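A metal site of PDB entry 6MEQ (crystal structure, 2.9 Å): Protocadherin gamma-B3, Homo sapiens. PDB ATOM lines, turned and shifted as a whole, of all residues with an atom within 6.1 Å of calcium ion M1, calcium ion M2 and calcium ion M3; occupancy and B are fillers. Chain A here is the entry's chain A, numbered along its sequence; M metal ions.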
ATOM      1  N   GLU A   9       7.490   4.052 -24.739  1.00  0.00           N
ATOM      2  CA  GLU A   9       8.560   3.114 -25.043  1.00  0.00           C
ATOM      3  C   GLU A   9       8.816   3.065 -26.543  1.00  0.00           C
ATOM      4  O   GLU A   9       8.067   3.633 -27.359  1.00  0.00           O
ATOM      5  CB  GLU A   9       8.224   1.728 -24.514  1.00  0.00           C
ATOM      6  CG  GLU A   9       6.913   1.161 -25.061  1.00  0.00           C
ATOM      7  CD  GLU A   9       6.771  -0.321 -24.815  1.00  0.00           C
ATOM      8  OE1 GLU A   9       7.808  -0.994 -24.631  1.00  0.00           O
ATOM      9  OE2 GLU A   9       5.624  -0.816 -24.806  1.00  0.00           O
ATOM     10  N   GLU A  10       9.894   2.370 -26.911  1.00  0.00           N
ATOM     11  CA  GLU A  10      10.260   2.135 -28.311  1.00  0.00           C
ATOM     12  C   GLU A  10      10.476   3.450 -29.060  1.00  0.00           C
ATOM     13  O   GLU A  10      10.139   3.581 -30.240  1.00  0.00           O
ATOM     14  CB  GLU A  10       9.223   1.274 -29.023  1.00  0.00           C
ATOM     15  CG  GLU A  10       8.968  -0.079 -28.357  1.00  0.00           C
ATOM     16  CD  GLU A  10      10.168  -1.005 -28.445  1.00  0.00           C
ATOM     17  OE1 GLU A  10      11.042  -0.780 -29.303  1.00  0.00           O
ATOM     18  OE2 GLU A  10      10.227  -1.960 -27.648  1.00  0.00           O
ATOM     19  N   ARG A  59      17.491   1.132 -27.067  1.00  0.00           N
ATOM     20  CA  ARG A  59      16.095   0.733 -27.185  1.00  0.00           C
ATOM     21  C   ARG A  59      15.517   0.426 -25.817  1.00  0.00           C
ATOM     22  O   ARG A  59      16.087  -0.344 -25.040  1.00  0.00           O
ATOM     23  CB  ARG A  59      15.973  -0.491 -28.102  1.00  0.00           C
ATOM     24  CG  ARG A  59      14.571  -1.047 -28.208  1.00  0.00           C
ATOM     25  CD  ARG A  59      14.508  -2.198 -29.207  1.00  0.00           C
ATOM     26  NE  ARG A  59      13.183  -2.817 -29.254  1.00  0.00           N
ATOM     27  CZ  ARG A  59      12.829  -3.878 -28.538  1.00  0.00           C
ATOM     28  NH1 ARG A  59      13.697  -4.450 -27.723  1.00  0.00           N
ATOM     29  NH2 ARG A  59      11.601  -4.373 -28.656  1.00  0.00           N
ATOM     30  N   ILE A  60      14.369   1.033 -25.514  1.00  0.00           N
ATOM     31  CA  ILE A  60      13.704   0.870 -24.230  1.00  0.00           C
ATOM     32  C   ILE A  60      12.476  -0.009 -24.473  1.00  0.00           C
ATOM     33  O   ILE A  60      11.435   0.472 -24.928  1.00  0.00           O
ATOM     34  CB  ILE A  60      13.316   2.219 -23.606  1.00  0.00           C
ATOM     35  CG1 ILE A  60      14.553   3.092 -23.432  1.00  0.00           C
ATOM     36  CG2 ILE A  60      12.613   2.007 -22.267  1.00  0.00           C
ATOM     37  CD1 ILE A  60      14.264   4.449 -22.828  1.00  0.00           C
ATOM     38  N   ASP A  61      12.607  -1.296 -24.178  1.00  0.00           N
ATOM     39  CA  ASP A  61      11.522  -2.255 -24.327  1.00  0.00           C
ATOM     40  C   ASP A  61      10.904  -2.497 -22.954  1.00  0.00           C
ATOM     41  O   ASP A  61      11.534  -3.092 -22.081  1.00  0.00           O
ATOM     42  CB  ASP A  61      12.025  -3.563 -24.942  1.00  0.00           C
ATOM     43  CG  ASP A  61      10.908  -4.528 -25.268  1.00  0.00           C
ATOM     44  OD1 ASP A  61       9.717  -4.126 -25.205  1.00  0.00           O
ATOM     45  OD2 ASP A  61      11.200  -5.697 -25.588  1.00  0.00           O
ATOM     46  N   ARG A  62       9.664  -2.034 -22.768  1.00  0.00           N
ATOM     47  CA  ARG A  62       9.018  -2.172 -21.465  1.00  0.00           C
ATOM     48  C   ARG A  62       8.755  -3.625 -21.113  1.00  0.00           C
ATOM     49  O   ARG A  62       8.765  -3.989 -19.926  1.00  0.00           O
ATOM     50  CB  ARG A  62       7.708  -1.377 -21.446  1.00  0.00           C
ATOM     51  CG  ARG A  62       7.117  -1.200 -20.060  1.00  0.00           C
ATOM     52  CD  ARG A  62       5.612  -1.057 -20.110  1.00  0.00           C
ATOM     53  NE  ARG A  62       4.980  -2.232 -20.692  1.00  0.00           N
ATOM     54  CZ  ARG A  62       4.690  -3.335 -20.009  1.00  0.00           C
ATOM     55  NH1 ARG A  62       4.966  -3.403 -18.715  1.00  0.00           N
ATOM     56  NH2 ARG A  62       4.115  -4.365 -20.620  1.00  0.00           N
ATOM     57  N   GLU A  63       8.515  -4.479 -22.111  1.00  0.00           N
ATOM     58  CA  GLU A  63       8.268  -5.890 -21.825  1.00  0.00           C
ATOM     59  C   GLU A  63       9.526  -6.596 -21.345  1.00  0.00           C
ATOM     60  O   GLU A  63       9.425  -7.579 -20.599  1.00  0.00           O
ATOM     61  CB  GLU A  63       7.703  -6.587 -23.077  1.00  0.00           C
ATOM     62  CG  GLU A  63       6.239  -6.310 -23.347  1.00  0.00           C
ATOM     63  CD  GLU A  63       5.975  -4.881 -23.775  1.00  0.00           C
ATOM     64  OE1 GLU A  63       6.790  -4.330 -24.553  1.00  0.00           O
ATOM     65  OE2 GLU A  63       4.953  -4.303 -23.331  1.00  0.00           O
ATOM     66  N   ASP A  95       3.463   2.396 -21.714  1.00  0.00           N
ATOM     67  CA  ASP A  95       3.283   1.180 -22.497  1.00  0.00           C
ATOM     68  C   ASP A  95       2.491   1.470 -23.765  1.00  0.00           C
ATOM     69  O   ASP A  95       1.478   2.179 -23.732  1.00  0.00           O
ATOM     70  CB  ASP A  95       2.574   0.106 -21.668  1.00  0.00           C
ATOM     71  CG  ASP A  95       2.292  -1.145 -22.478  1.00  0.00           C
ATOM     72  OD1 ASP A  95       3.254  -1.821 -22.886  1.00  0.00           O
ATOM     73  OD2 ASP A  95       1.101  -1.450 -22.699  1.00  0.00           O
ATOM     74  N   ILE A  96       2.958   0.916 -24.879  1.00  0.00           N
ATOM     75  CA  ILE A  96       2.267   1.015 -26.154  1.00  0.00           C
ATOM     76  C   ILE A  96       1.848  -0.388 -26.584  1.00  0.00           C
ATOM     77  O   ILE A  96       2.423  -1.391 -26.157  1.00  0.00           O
ATOM     78  CB  ILE A  96       3.133   1.680 -27.242  1.00  0.00           C
ATOM     79  CG1 ILE A  96       4.334   0.800 -27.584  1.00  0.00           C
ATOM     80  CG2 ILE A  96       3.576   3.062 -26.803  1.00  0.00           C
ATOM     81  CD1 ILE A  96       5.220   1.371 -28.680  1.00  0.00           C
ATOM     82  N   ASN A  97       0.821  -0.442 -27.433  1.00  0.00           N
ATOM     83  CA  ASN A  97       0.288  -1.710 -27.921  1.00  0.00           C
ATOM     84  C   ASN A  97       1.095  -2.128 -29.150  1.00  0.00           C
ATOM     85  O   ASN A  97       0.692  -1.941 -30.300  1.00  0.00           O
ATOM     86  CB  ASN A  97      -1.196  -1.599 -28.228  1.00  0.00           C
ATOM     87  CG  ASN A  97      -1.810  -2.924 -28.606  1.00  0.00           C
ATOM     88  OD1 ASN A  97      -1.304  -3.978 -28.248  1.00  0.00           O
ATOM     89  ND2 ASN A  97      -2.922  -2.878 -29.345  1.00  0.00           N
ATOM     90  N   ASP A  98       2.263  -2.716 -28.890  1.00  0.00           N
ATOM     91  CA  ASP A  98       3.156  -3.174 -29.947  1.00  0.00           C
ATOM     92  C   ASP A  98       3.360  -4.685 -29.920  1.00  0.00           C
ATOM     93  O   ASP A  98       4.285  -5.199 -30.551  1.00  0.00           O
ATOM     94  CB  ASP A  98       4.507  -2.454 -29.856  1.00  0.00           C
ATOM     95  CG  ASP A  98       5.150  -2.590 -28.491  1.00  0.00           C
ATOM     96  OD1 ASP A  98       4.506  -3.120 -27.573  1.00  0.00           O
ATOM     97  OD2 ASP A  98       6.315  -2.160 -28.348  1.00  0.00           O
ATOM     98  N   ASN A  99       2.502  -5.412 -29.198  1.00  0.00           N
ATOM     99  CA  ASN A  99       2.612  -6.859 -29.110  1.00  0.00           C
ATOM    100  C   ASN A  99       1.234  -7.503 -29.230  1.00  0.00           C
ATOM    101  O   ASN A  99       0.358  -7.236 -28.396  1.00  0.00           O
ATOM    102  CB  ASN A  99       3.280  -7.271 -27.796  1.00  0.00           C
ATOM    103  CG  ASN A  99       4.754  -6.899 -27.756  1.00  0.00           C
ATOM    104  OD1 ASN A  99       5.177  -6.093 -26.927  1.00  0.00           O
ATOM    105  ND2 ASN A  99       5.545  -7.496 -28.644  1.00  0.00           N
ATOM    106  N   PRO A 100       1.015  -8.344 -30.229  1.00  0.00           N
ATOM    107  CA  PRO A 100      -0.294  -8.984 -30.388  1.00  0.00           C
ATOM    108  C   PRO A 100      -0.471 -10.119 -29.401  1.00  0.00           C
ATOM    109  O   PRO A 100       0.526 -10.689 -28.921  1.00  0.00           O
ATOM    110  CB  PRO A 100      -0.247  -9.502 -31.834  1.00  0.00           C
ATOM    111  CG  PRO A 100       1.191  -9.764 -32.079  1.00  0.00           C
ATOM    112  CD  PRO A 100       1.944  -8.707 -31.311  1.00  0.00           C
ATOM    113  N   PRO A 101      -1.704 -10.462 -29.060  1.00  0.00           N
ATOM    114  CA  PRO A 101      -1.930 -11.624 -28.190  1.00  0.00           C
ATOM    115  C   PRO A 101      -1.611 -12.921 -28.928  1.00  0.00           C
ATOM    116  O   PRO A 101      -1.431 -12.955 -30.143  1.00  0.00           O
ATOM    117  CB  PRO A 101      -3.413 -11.524 -27.848  1.00  0.00           C
ATOM    118  CG  PRO A 101      -4.012 -10.764 -28.984  1.00  0.00           C
ATOM    119  CD  PRO A 101      -2.962  -9.786 -29.416  1.00  0.00           C
ATOM    120  N   ASP A 129      -0.862 -11.862 -23.371  1.00  0.00           N
ATOM    121  CA  ASP A 129      -0.307 -10.682 -24.016  1.00  0.00           C
ATOM    122  C   ASP A 129       0.776 -10.084 -23.130  1.00  0.00           C
ATOM    123  O   ASP A 129       0.521  -9.773 -21.959  1.00  0.00           O
ATOM    124  CB  ASP A 129      -1.417  -9.664 -24.280  1.00  0.00           C
ATOM    125  CG  ASP A 129      -1.017  -8.620 -25.314  1.00  0.00           C
ATOM    126  OD1 ASP A 129       0.108  -8.088 -25.236  1.00  0.00           O
ATOM    127  OD2 ASP A 129      -1.842  -8.326 -26.208  1.00  0.00           O
ATOM    128  N   PRO A 130       1.999  -9.913 -23.644  1.00  0.00           N
ATOM    129  CA  PRO A 130       3.074  -9.352 -22.809  1.00  0.00           C
ATOM    130  C   PRO A 130       2.867  -7.890 -22.434  1.00  0.00           C
ATOM    131  O   PRO A 130       3.606  -7.377 -21.594  1.00  0.00           O
ATOM    132  CB  PRO A 130       4.323  -9.524 -23.689  1.00  0.00           C
ATOM    133  CG  PRO A 130       3.798  -9.586 -25.076  1.00  0.00           C
ATOM    134  CD  PRO A 130       2.467 -10.281 -24.993  1.00  0.00           C
ATOM    135  N   ASP A 131       1.891  -7.206 -23.030  1.00  0.00           N
ATOM    136  CA  ASP A 131       1.604  -5.819 -22.686  1.00  0.00           C
ATOM    137  C   ASP A 131       0.852  -5.761 -21.354  1.00  0.00           C
ATOM    138  O   ASP A 131       0.550  -6.777 -20.731  1.00  0.00           O
ATOM    139  CB  ASP A 131       0.815  -5.147 -23.806  1.00  0.00           C
ATOM    140  CG  ASP A 131       1.567  -5.118 -25.124  1.00  0.00           C
ATOM    141  OD1 ASP A 131       2.810  -5.016 -25.090  1.00  0.00           O
ATOM    142  OD2 ASP A 131       0.913  -5.199 -26.182  1.00  0.00           O
ATOM    143  N   VAL A 132       0.552  -4.543 -20.912  1.00  0.00           N
ATOM    144  CA  VAL A 132      -0.180  -4.306 -19.673  1.00  0.00           C
ATOM    145  C   VAL A 132      -1.284  -3.296 -19.947  1.00  0.00           C
ATOM    146  O   VAL A 132      -1.353  -2.687 -21.015  1.00  0.00           O
ATOM    147  CB  VAL A 132       0.739  -3.815 -18.536  1.00  0.00           C
ATOM    148  CG1 VAL A 132       1.763  -4.878 -18.166  1.00  0.00           C
ATOM    149  CG2 VAL A 132       1.421  -2.509 -18.925  1.00  0.00           C
ATOM    150  N   ASN A 135      -3.897  -2.498 -23.201  1.00  0.00           N
ATOM    151  CA  ASN A 135      -3.214  -3.143 -24.324  1.00  0.00           C
ATOM    152  C   ASN A 135      -3.201  -4.654 -24.197  1.00  0.00           C
ATOM    153  O   ASN A 135      -2.989  -5.343 -25.196  1.00  0.00           O
ATOM    154  CB  ASN A 135      -1.784  -2.618 -24.444  1.00  0.00           C
ATOM    155  CG  ASN A 135      -1.721  -1.110 -24.612  1.00  0.00           C
ATOM    156  OD1 ASN A 135      -2.644  -0.504 -25.156  1.00  0.00           O
ATOM    157  ND2 ASN A 135      -0.642  -0.506 -24.144  1.00  0.00           N
ATOM    158  N   SER A 136      -3.438  -5.191 -22.998  1.00  0.00           N
ATOM    159  CA  SER A 136      -3.517  -6.624 -22.783  1.00  0.00           C
ATOM    160  C   SER A 136      -4.934  -7.108 -22.467  1.00  0.00           C
ATOM    161  O   SER A 136      -5.149  -8.315 -22.378  1.00  0.00           O
ATOM    162  CB  SER A 136      -2.583  -7.049 -21.649  1.00  0.00           C
ATOM    163  OG  SER A 136      -2.933  -6.422 -20.426  1.00  0.00           O
ATOM    164  N   GLN A 138      -8.093  -8.504 -23.231  1.00  0.00           N
ATOM    165  CA  GLN A 138      -8.528  -9.244 -24.406  1.00  0.00           C
ATOM    166  C   GLN A 138     -10.057  -9.268 -24.500  1.00  0.00           C
ATOM    167  O   GLN A 138     -10.766  -9.210 -23.501  1.00  0.00           O
ATOM    168  CB  GLN A 138      -8.001 -10.676 -24.365  1.00  0.00           C
ATOM    169  CG  GLN A 138      -6.487 -10.766 -24.259  1.00  0.00           C
ATOM    170  CD  GLN A 138      -5.772 -10.108 -25.420  1.00  0.00           C
ATOM    171  OE1 GLN A 138      -6.269 -10.101 -26.548  1.00  0.00           O
ATOM    172  NE2 GLN A 138      -4.598  -9.553 -25.143  1.00  0.00           N
ATOM    173  N   ASP A 186      -7.332  -7.418 -28.465  1.00  0.00           N
ATOM    174  CA  ASP A 186      -7.000  -6.592 -27.312  1.00  0.00           C
ATOM    175  C   ASP A 186      -7.635  -5.207 -27.452  1.00  0.00           C
ATOM    176  O   ASP A 186      -8.149  -4.827 -28.512  1.00  0.00           O
ATOM    177  CB  ASP A 186      -5.484  -6.478 -27.142  1.00  0.00           C
ATOM    178  CG  ASP A 186      -4.790  -5.909 -28.366  1.00  0.00           C
ATOM    179  OD1 ASP A 186      -5.477  -5.584 -29.360  1.00  0.00           O
ATOM    180  OD2 ASP A 186      -3.543  -5.782 -28.331  1.00  0.00           O
ATOM    181  N   ARG A 192      -4.582  -5.346 -32.223  1.00  0.00           N
ATOM    182  CA  ARG A 192      -3.931  -6.558 -32.705  1.00  0.00           C
ATOM    183  C   ARG A 192      -4.708  -7.772 -32.230  1.00  0.00           C
ATOM    184  O   ARG A 192      -5.230  -7.790 -31.110  1.00  0.00           O
ATOM    185  CB  ARG A 192      -2.487  -6.625 -32.228  1.00  0.00           C
ATOM    186  CG  ARG A 192      -1.548  -5.667 -32.960  1.00  0.00           C
ATOM    187  CD  ARG A 192      -0.134  -5.745 -32.399  1.00  0.00           C
ATOM    188  NE  ARG A 192       0.835  -5.072 -33.259  1.00  0.00           N
ATOM    189  CZ  ARG A 192       1.083  -3.773 -33.223  1.00  0.00           C
ATOM    190  NH1 ARG A 192       0.436  -2.992 -32.366  1.00  0.00           N
ATOM    191  NH2 ARG A 192       1.987  -3.244 -34.041  1.00  0.00           N
HETATM  192 CA    CA M   1      -1.284  -6.023 -26.851  1.00  0.00          CA
HETATM  193 CA    CA M   2       4.169  -2.820 -25.076  1.00  0.00          CA
HETATM  194 CA    CA M   3       7.823  -3.165 -26.528  1.00  0.00          CA
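The side-chain amide oxygen (OD1) of Asn 99 sits close to the side-chain carboxylate (OE1) of Glu 63 (3.4 Å). OD2 of Asp 95 sits at hydrogen-bond distance from ND2 of Asn 135 (2.5 Å). OD1 of Asp 95 sits close to NE of Arg 62 (2.8 Å). The backbone NH (N) of Asp 186 sits at hydrogen-bond distance from the side-chain amide oxygen (OE1) of Gln 138, at 3.5 Å. NH2 of Arg 59 is in salt-bridge range of OE2 of Glu 10 (3.0 Å). The side-chain carboxylate (OD1) of Asp 98 sits close to the side-chain amide oxygen (OD1) of Asn 99. The side-chain carboxylate of Glu 9 sits close to the backbone NH of Arg 62 (2.8 Å). The side-chain carboxylate of Asp 186 sits at hydrogen-bond distance from the backbone NH of Arg 192 (3.0 Å).
Of the 23 residues printed, 6 come within 4 Å of calcium ion M1. The nearest printed residue that does not touch calcium ion M1 is Ser 136 (4.5 Å).
Within 4 Å of calcium ion M2: Glu 9, Glu 63, Asp 95, Ile 96, Asp 98, Asn 99 and Asp 131.
Within 4 Å of calcium ion M3: Glu 9, Glu 10, Asp 61, Glu 63, Asp 98 and Asn 99.
Calcium ion M1 is bound by OD2 of Asp 131 (2.4 Å), OD2 of Asp 129 (2.5 Å), O of Asn 135 (2.5 Å), OD1 of Asn 97 (2.5 Å), O of Asn 99 (2.6 Å) and OD2 of Asp 186 (2.7 Å). Slightly farther from calcium ion M1 lies the side-chain carboxylate (OD1) of Asp 129 (3.0 Å).
Calcium ion M2 is bound by OE2 of Glu 63 (2.4 Å). Calcium ion M2 is bound by OE2 of Glu 9, at 2.5 Å. O of Ile 96 binds calcium ion M2 (2.5 Å). Calcium ion M2 is bound by the side-chain carboxylate (OD1) of Asp 98, at 2.5 Å. OD1 of Asp 95 is bound to calcium ion M2, 2.6 Å away. OD1 of Asp 131 is bound to calcium ion M2 (2.6 Å). Calcium ion M2 has six donor atoms within binding distance. Slightly farther from calcium ion M2 lies the side-chain carboxylate (OE1) of Glu 63 (3.1 Å).
Calcium ion M3 is bound by the side-chain carboxylate (OD1) of Asp 61 (2.5 Å), the side-chain carboxylate (OE1) of Glu 63 (2.5 Å), the side-chain carboxylate (OD2) of Asp 98 (2.6 Å) and the side-chain carboxylate (OE1) of Glu 9 (2.9 Å). Calcium ion M3 has four donor atoms within binding distance. Slightly farther from calcium ion M3 lies OE2 of Glu 10 (2.9 Å).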
